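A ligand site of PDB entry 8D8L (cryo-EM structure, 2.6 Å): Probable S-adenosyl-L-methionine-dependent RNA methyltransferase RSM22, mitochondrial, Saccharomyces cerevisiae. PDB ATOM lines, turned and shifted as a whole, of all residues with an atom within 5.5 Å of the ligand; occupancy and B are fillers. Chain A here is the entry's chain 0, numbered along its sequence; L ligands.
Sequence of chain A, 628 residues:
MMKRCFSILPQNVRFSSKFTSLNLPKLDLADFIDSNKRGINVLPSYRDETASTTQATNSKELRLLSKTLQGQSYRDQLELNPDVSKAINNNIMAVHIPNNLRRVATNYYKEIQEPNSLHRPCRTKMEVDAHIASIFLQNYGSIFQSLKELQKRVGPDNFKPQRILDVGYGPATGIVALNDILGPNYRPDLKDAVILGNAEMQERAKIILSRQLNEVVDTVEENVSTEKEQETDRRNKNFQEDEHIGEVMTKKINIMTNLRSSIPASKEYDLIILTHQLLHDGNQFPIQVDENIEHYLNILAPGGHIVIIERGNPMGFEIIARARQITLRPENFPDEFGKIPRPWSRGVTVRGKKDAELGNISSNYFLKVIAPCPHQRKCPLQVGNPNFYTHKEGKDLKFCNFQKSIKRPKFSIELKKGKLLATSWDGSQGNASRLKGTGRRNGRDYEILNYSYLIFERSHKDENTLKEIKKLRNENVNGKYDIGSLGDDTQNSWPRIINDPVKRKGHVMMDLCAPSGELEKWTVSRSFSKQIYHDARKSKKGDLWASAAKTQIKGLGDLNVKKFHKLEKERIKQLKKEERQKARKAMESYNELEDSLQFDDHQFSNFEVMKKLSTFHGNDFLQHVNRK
An iron atom (FE3) of the ligand is bound by the side-chain sulfur (SG) of Cys 513. The side-chain sulfur (SG) of Cys 373 binds an iron atom (FE2) of the ligand, at 2.2 Å. SG of Cys 400 is bound to FE1 of the ligand, at 2.3 Å. The side-chain sulfur (SG) of Cys 379 is bound to an iron atom (FE4) of the ligand (2.3 Å). NE2 of His 375 sits close to S1 of the ligand (3.6 Å).
The backbone carbonyl oxygen of Arg 496 lies within hydrogen-bond range of the backbone NH of Cys 513 (2.9 Å). SG of Cys 379 lies close to N of Leu 381 (3.5 Å). The backbone carbonyl oxygen of His 375 sits at hydrogen-bond distance from the guanidinium group of Arg 324, at 3.0 Å.
A sulfur (S4) of the ligand sits close to the backbone carbonyl oxygen (O) of Pro 372, at 3.5 Å. Residues that only touch the ligand: Arg 324 (3.8 Å), Pro 380 (3.9 Å) and Leu 381 (3.9 Å). Hydrophobic or aromatic side chains within 4 Å of the ligand: His 375, Pro 380 and Leu 381. Of the 16 residues printed, 9 come within 4 Å of the ligand. Along chain A the residues within 4 Å of the ligand span positions 324 to 513. The nearest printed residue that does not touch the ligand is Phe 317 (4.1 Å).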
ATOM      1  N   PHE A 317      18.543   1.645   2.494  1.00  0.00           N
ATOM      2  CA  PHE A 317      18.344   3.012   2.950  1.00  0.00           C
ATOM      3  C   PHE A 317      17.288   3.057   4.040  1.00  0.00           C
ATOM      4  O   PHE A 317      17.426   3.801   5.009  1.00  0.00           O
ATOM      5  CB  PHE A 317      17.922   3.921   1.793  1.00  0.00           C
ATOM      6  CG  PHE A 317      17.231   5.162   2.248  1.00  0.00           C
ATOM      7  CD1 PHE A 317      17.871   6.073   3.063  1.00  0.00           C
ATOM      8  CD2 PHE A 317      15.931   5.417   1.884  1.00  0.00           C
ATOM      9  CE1 PHE A 317      17.233   7.201   3.491  1.00  0.00           C
ATOM     10  CE2 PHE A 317      15.286   6.552   2.302  1.00  0.00           C
ATOM     11  CZ  PHE A 317      15.940   7.449   3.107  1.00  0.00           C
ATOM     12  N   ILE A 320      18.929   2.006   7.328  1.00  0.00           N
ATOM     13  CA  ILE A 320      19.681   3.121   7.927  1.00  0.00           C
ATOM     14  C   ILE A 320      18.774   4.227   8.429  1.00  0.00           C
ATOM     15  O   ILE A 320      19.035   4.829   9.473  1.00  0.00           O
ATOM     16  CB  ILE A 320      20.770   3.685   6.983  1.00  0.00           C
ATOM     17  CG1 ILE A 320      21.855   2.652   6.685  1.00  0.00           C
ATOM     18  CG2 ILE A 320      21.335   5.004   7.508  1.00  0.00           C
ATOM     19  CD1 ILE A 320      21.616   1.802   5.563  1.00  0.00           C
ATOM     20  N   ARG A 324      18.758   5.409  12.248  1.00  0.00           N
ATOM     21  CA  ARG A 324      18.964   6.803  12.610  1.00  0.00           C
ATOM     22  C   ARG A 324      17.822   7.309  13.473  1.00  0.00           C
ATOM     23  O   ARG A 324      18.047   7.993  14.480  1.00  0.00           O
ATOM     24  CB  ARG A 324      19.076   7.640  11.336  1.00  0.00           C
ATOM     25  CG  ARG A 324      19.755   8.963  11.497  1.00  0.00           C
ATOM     26  CD  ARG A 324      19.750   9.696  10.172  1.00  0.00           C
ATOM     27  NE  ARG A 324      18.681  10.680  10.076  1.00  0.00           N
ATOM     28  CZ  ARG A 324      18.799  11.961  10.391  1.00  0.00           C
ATOM     29  NH1 ARG A 324      19.945  12.482  10.808  1.00  0.00           N
ATOM     30  NH2 ARG A 324      17.749  12.758  10.270  1.00  0.00           N
ATOM     31  N   PRO A 372      26.439  10.129   7.097  1.00  0.00           N
ATOM     32  CA  PRO A 372      26.456  11.182   6.090  1.00  0.00           C
ATOM     33  C   PRO A 372      25.509  12.336   6.395  1.00  0.00           C
ATOM     34  O   PRO A 372      25.383  13.245   5.597  1.00  0.00           O
ATOM     35  CB  PRO A 372      25.990  10.450   4.831  1.00  0.00           C
ATOM     36  CG  PRO A 372      25.100   9.403   5.340  1.00  0.00           C
ATOM     37  CD  PRO A 372      25.693   8.944   6.633  1.00  0.00           C
ATOM     38  N   CYS A 373      24.863  12.297   7.525  1.00  0.00           N
ATOM     39  CA  CYS A 373      23.802  13.258   7.766  1.00  0.00           C
ATOM     40  C   CYS A 373      24.388  14.522   8.377  1.00  0.00           C
ATOM     41  O   CYS A 373      25.155  14.447   9.329  1.00  0.00           O
ATOM     42  CB  CYS A 373      22.765  12.641   8.677  1.00  0.00           C
ATOM     43  SG  CYS A 373      22.272  11.016   8.116  1.00  0.00           S
ATOM     44  N   PRO A 374      24.081  15.702   7.825  1.00  0.00           N
ATOM     45  CA  PRO A 374      24.525  16.958   8.451  1.00  0.00           C
ATOM     46  C   PRO A 374      23.556  17.549   9.462  1.00  0.00           C
ATOM     47  O   PRO A 374      23.739  18.706   9.844  1.00  0.00           O
ATOM     48  CB  PRO A 374      24.662  17.879   7.238  1.00  0.00           C
ATOM     49  CG  PRO A 374      23.565  17.464   6.383  1.00  0.00           C
ATOM     50  CD  PRO A 374      23.436  15.971   6.535  1.00  0.00           C
ATOM     51  N   HIS A 375      22.561  16.783   9.902  1.00  0.00           N
ATOM     52  CA  HIS A 375      21.623  17.257  10.909  1.00  0.00           C
ATOM     53  C   HIS A 375      21.134  16.045  11.687  1.00  0.00           C
ATOM     54  O   HIS A 375      21.542  14.910  11.435  1.00  0.00           O
ATOM     55  CB  HIS A 375      20.464  18.012  10.268  1.00  0.00           C
ATOM     56  CG  HIS A 375      19.705  17.215   9.269  1.00  0.00           C
ATOM     57  ND1 HIS A 375      19.842  17.400   7.910  1.00  0.00           N
ATOM     58  CD2 HIS A 375      18.800  16.213   9.411  1.00  0.00           C
ATOM     59  CE1 HIS A 375      19.062  16.556   7.270  1.00  0.00           C
ATOM     60  NE2 HIS A 375      18.411  15.832   8.155  1.00  0.00           N
ATOM     61  N   LYS A 378      14.339  14.936  11.104  1.00  0.00           N
ATOM     62  CA  LYS A 378      13.773  13.838  10.325  1.00  0.00           C
ATOM     63  C   LYS A 378      14.448  13.755   8.961  1.00  0.00           C
ATOM     64  O   LYS A 378      14.607  14.758   8.267  1.00  0.00           O
ATOM     65  CB  LYS A 378      12.265  14.040  10.160  1.00  0.00           C
ATOM     66  CG  LYS A 378      11.587  12.958   9.342  1.00  0.00           C
ATOM     67  CD  LYS A 378      10.083  13.148   9.294  1.00  0.00           C
ATOM     68  CE  LYS A 378       9.434  12.129   8.381  1.00  0.00           C
ATOM     69  NZ  LYS A 378       9.614  10.727   8.847  1.00  0.00           N
ATOM     70  N   CYS A 379      14.818  12.541   8.570  1.00  0.00           N
ATOM     71  CA  CYS A 379      15.430  12.350   7.263  1.00  0.00           C
ATOM     72  C   CYS A 379      14.424  12.725   6.180  1.00  0.00           C
ATOM     73  O   CYS A 379      13.313  12.191   6.157  1.00  0.00           O
ATOM     74  CB  CYS A 379      15.872  10.908   7.070  1.00  0.00           C
ATOM     75  SG  CYS A 379      16.349  10.509   5.375  1.00  0.00           S
ATOM     76  N   PRO A 380      14.775  13.631   5.255  1.00  0.00           N
ATOM     77  CA  PRO A 380      13.787  14.083   4.273  1.00  0.00           C
ATOM     78  C   PRO A 380      13.339  13.004   3.297  1.00  0.00           C
ATOM     79  O   PRO A 380      12.244  13.130   2.729  1.00  0.00           O
ATOM     80  CB  PRO A 380      14.503  15.225   3.556  1.00  0.00           C
ATOM     81  CG  PRO A 380      15.930  14.907   3.697  1.00  0.00           C
ATOM     82  CD  PRO A 380      16.072  14.291   5.046  1.00  0.00           C
ATOM     83  N   LEU A 381      14.119  11.946   3.096  1.00  0.00           N
ATOM     84  CA  LEU A 381      13.810  10.951   2.081  1.00  0.00           C
ATOM     85  C   LEU A 381      13.079   9.728   2.624  1.00  0.00           C
ATOM     86  O   LEU A 381      12.699   8.853   1.841  1.00  0.00           O
ATOM     87  CB  LEU A 381      15.095  10.486   1.394  1.00  0.00           C
ATOM     88  CG  LEU A 381      15.749  11.483   0.440  1.00  0.00           C
ATOM     89  CD1 LEU A 381      17.047  10.932  -0.127  1.00  0.00           C
ATOM     90  CD2 LEU A 381      14.815  11.865  -0.688  1.00  0.00           C
ATOM     91  N   CYS A 400      18.602   7.500  -0.112  1.00  0.00           N
ATOM     92  CA  CYS A 400      19.950   7.970   0.178  1.00  0.00           C
ATOM     93  C   CYS A 400      20.921   6.800   0.103  1.00  0.00           C
ATOM     94  O   CYS A 400      21.007   5.984   1.025  1.00  0.00           O
ATOM     95  CB  CYS A 400      19.998   8.622   1.564  1.00  0.00           C
ATOM     96  SG  CYS A 400      21.525   9.519   1.917  1.00  0.00           S
ATOM     97  N   PHE A 402      25.131   5.956  -1.632  1.00  0.00           N
ATOM     98  CA  PHE A 402      26.378   6.565  -2.079  1.00  0.00           C
ATOM     99  C   PHE A 402      27.148   5.544  -2.883  1.00  0.00           C
ATOM    100  O   PHE A 402      26.997   4.334  -2.708  1.00  0.00           O
ATOM    101  CB  PHE A 402      27.196   7.087  -0.895  1.00  0.00           C
ATOM    102  CG  PHE A 402      26.510   8.186  -0.145  1.00  0.00           C
ATOM    103  CD1 PHE A 402      26.649   9.498  -0.549  1.00  0.00           C
ATOM    104  CD2 PHE A 402      25.688   7.903   0.928  1.00  0.00           C
ATOM    105  CE1 PHE A 402      26.023  10.510   0.128  1.00  0.00           C
ATOM    106  CE2 PHE A 402      25.048   8.914   1.605  1.00  0.00           C
ATOM    107  CZ  PHE A 402      25.201  10.217   1.204  1.00  0.00           C
ATOM    108  N   ARG A 496      25.258  18.033   2.534  1.00  0.00           N
ATOM    109  CA  ARG A 496      25.725  16.773   1.974  1.00  0.00           C
ATOM    110  C   ARG A 496      25.247  16.718   0.530  1.00  0.00           C
ATOM    111  O   ARG A 496      24.040  16.816   0.290  1.00  0.00           O
ATOM    112  CB  ARG A 496      25.130  15.599   2.744  1.00  0.00           C
ATOM    113  CG  ARG A 496      25.568  14.190   2.369  1.00  0.00           C
ATOM    114  CD  ARG A 496      26.781  13.696   3.154  1.00  0.00           C
ATOM    115  NE  ARG A 496      28.111  13.880   2.600  1.00  0.00           N
ATOM    116  CZ  ARG A 496      29.221  13.607   3.263  1.00  0.00           C
ATOM    117  NH1 ARG A 496      29.204  13.247   4.535  1.00  0.00           N
ATOM    118  NH2 ARG A 496      30.393  13.690   2.641  1.00  0.00           N
ATOM    119  N   ILE A 498      24.048  14.697  -2.367  1.00  0.00           N
ATOM    120  CA  ILE A 498      23.416  13.381  -2.417  1.00  0.00           C
ATOM    121  C   ILE A 498      22.938  13.025  -3.812  1.00  0.00           C
ATOM    122  O   ILE A 498      22.244  12.024  -3.985  1.00  0.00           O
ATOM    123  CB  ILE A 498      22.258  13.295  -1.398  1.00  0.00           C
ATOM    124  CG1 ILE A 498      21.293  14.460  -1.590  1.00  0.00           C
ATOM    125  CG2 ILE A 498      22.802  13.299   0.013  1.00  0.00           C
ATOM    126  CD1 ILE A 498      19.898  14.140  -1.186  1.00  0.00           C
ATOM    127  N   CYS A 513      21.343  17.436   1.009  1.00  0.00           N
ATOM    128  CA  CYS A 513      20.678  17.213   2.283  1.00  0.00           C
ATOM    129  C   CYS A 513      21.263  18.242   3.228  1.00  0.00           C
ATOM    130  O   CYS A 513      22.403  18.109   3.680  1.00  0.00           O
ATOM    131  CB  CYS A 513      20.894  15.791   2.780  1.00  0.00           C
ATOM    132  SG  CYS A 513      19.925  15.396   4.216  1.00  0.00           S
HETATM  133 FE1  LIG L   1      20.744  10.783   3.624  1.00  0.00          FE
HETATM  134 FE2  LIG L   1      20.978  11.362   6.310  1.00  0.00          FE
HETATM  135 FE3  LIG L   1      20.084  13.207   4.605  1.00  0.00          FE
HETATM  136 FE4  LIG L   1      18.539  11.077   5.193  1.00  0.00          FE
HETATM  137  S1  LIG L   1      19.219  12.670   6.674  1.00  0.00           S
HETATM  138  S2  LIG L   1      18.916  11.932   3.091  1.00  0.00           S
HETATM  139  S3  LIG L   1      20.103   9.444   5.405  1.00  0.00           S
HETATM  140  S4  LIG L   1      22.137  12.331   4.566  1.00  0.00           S
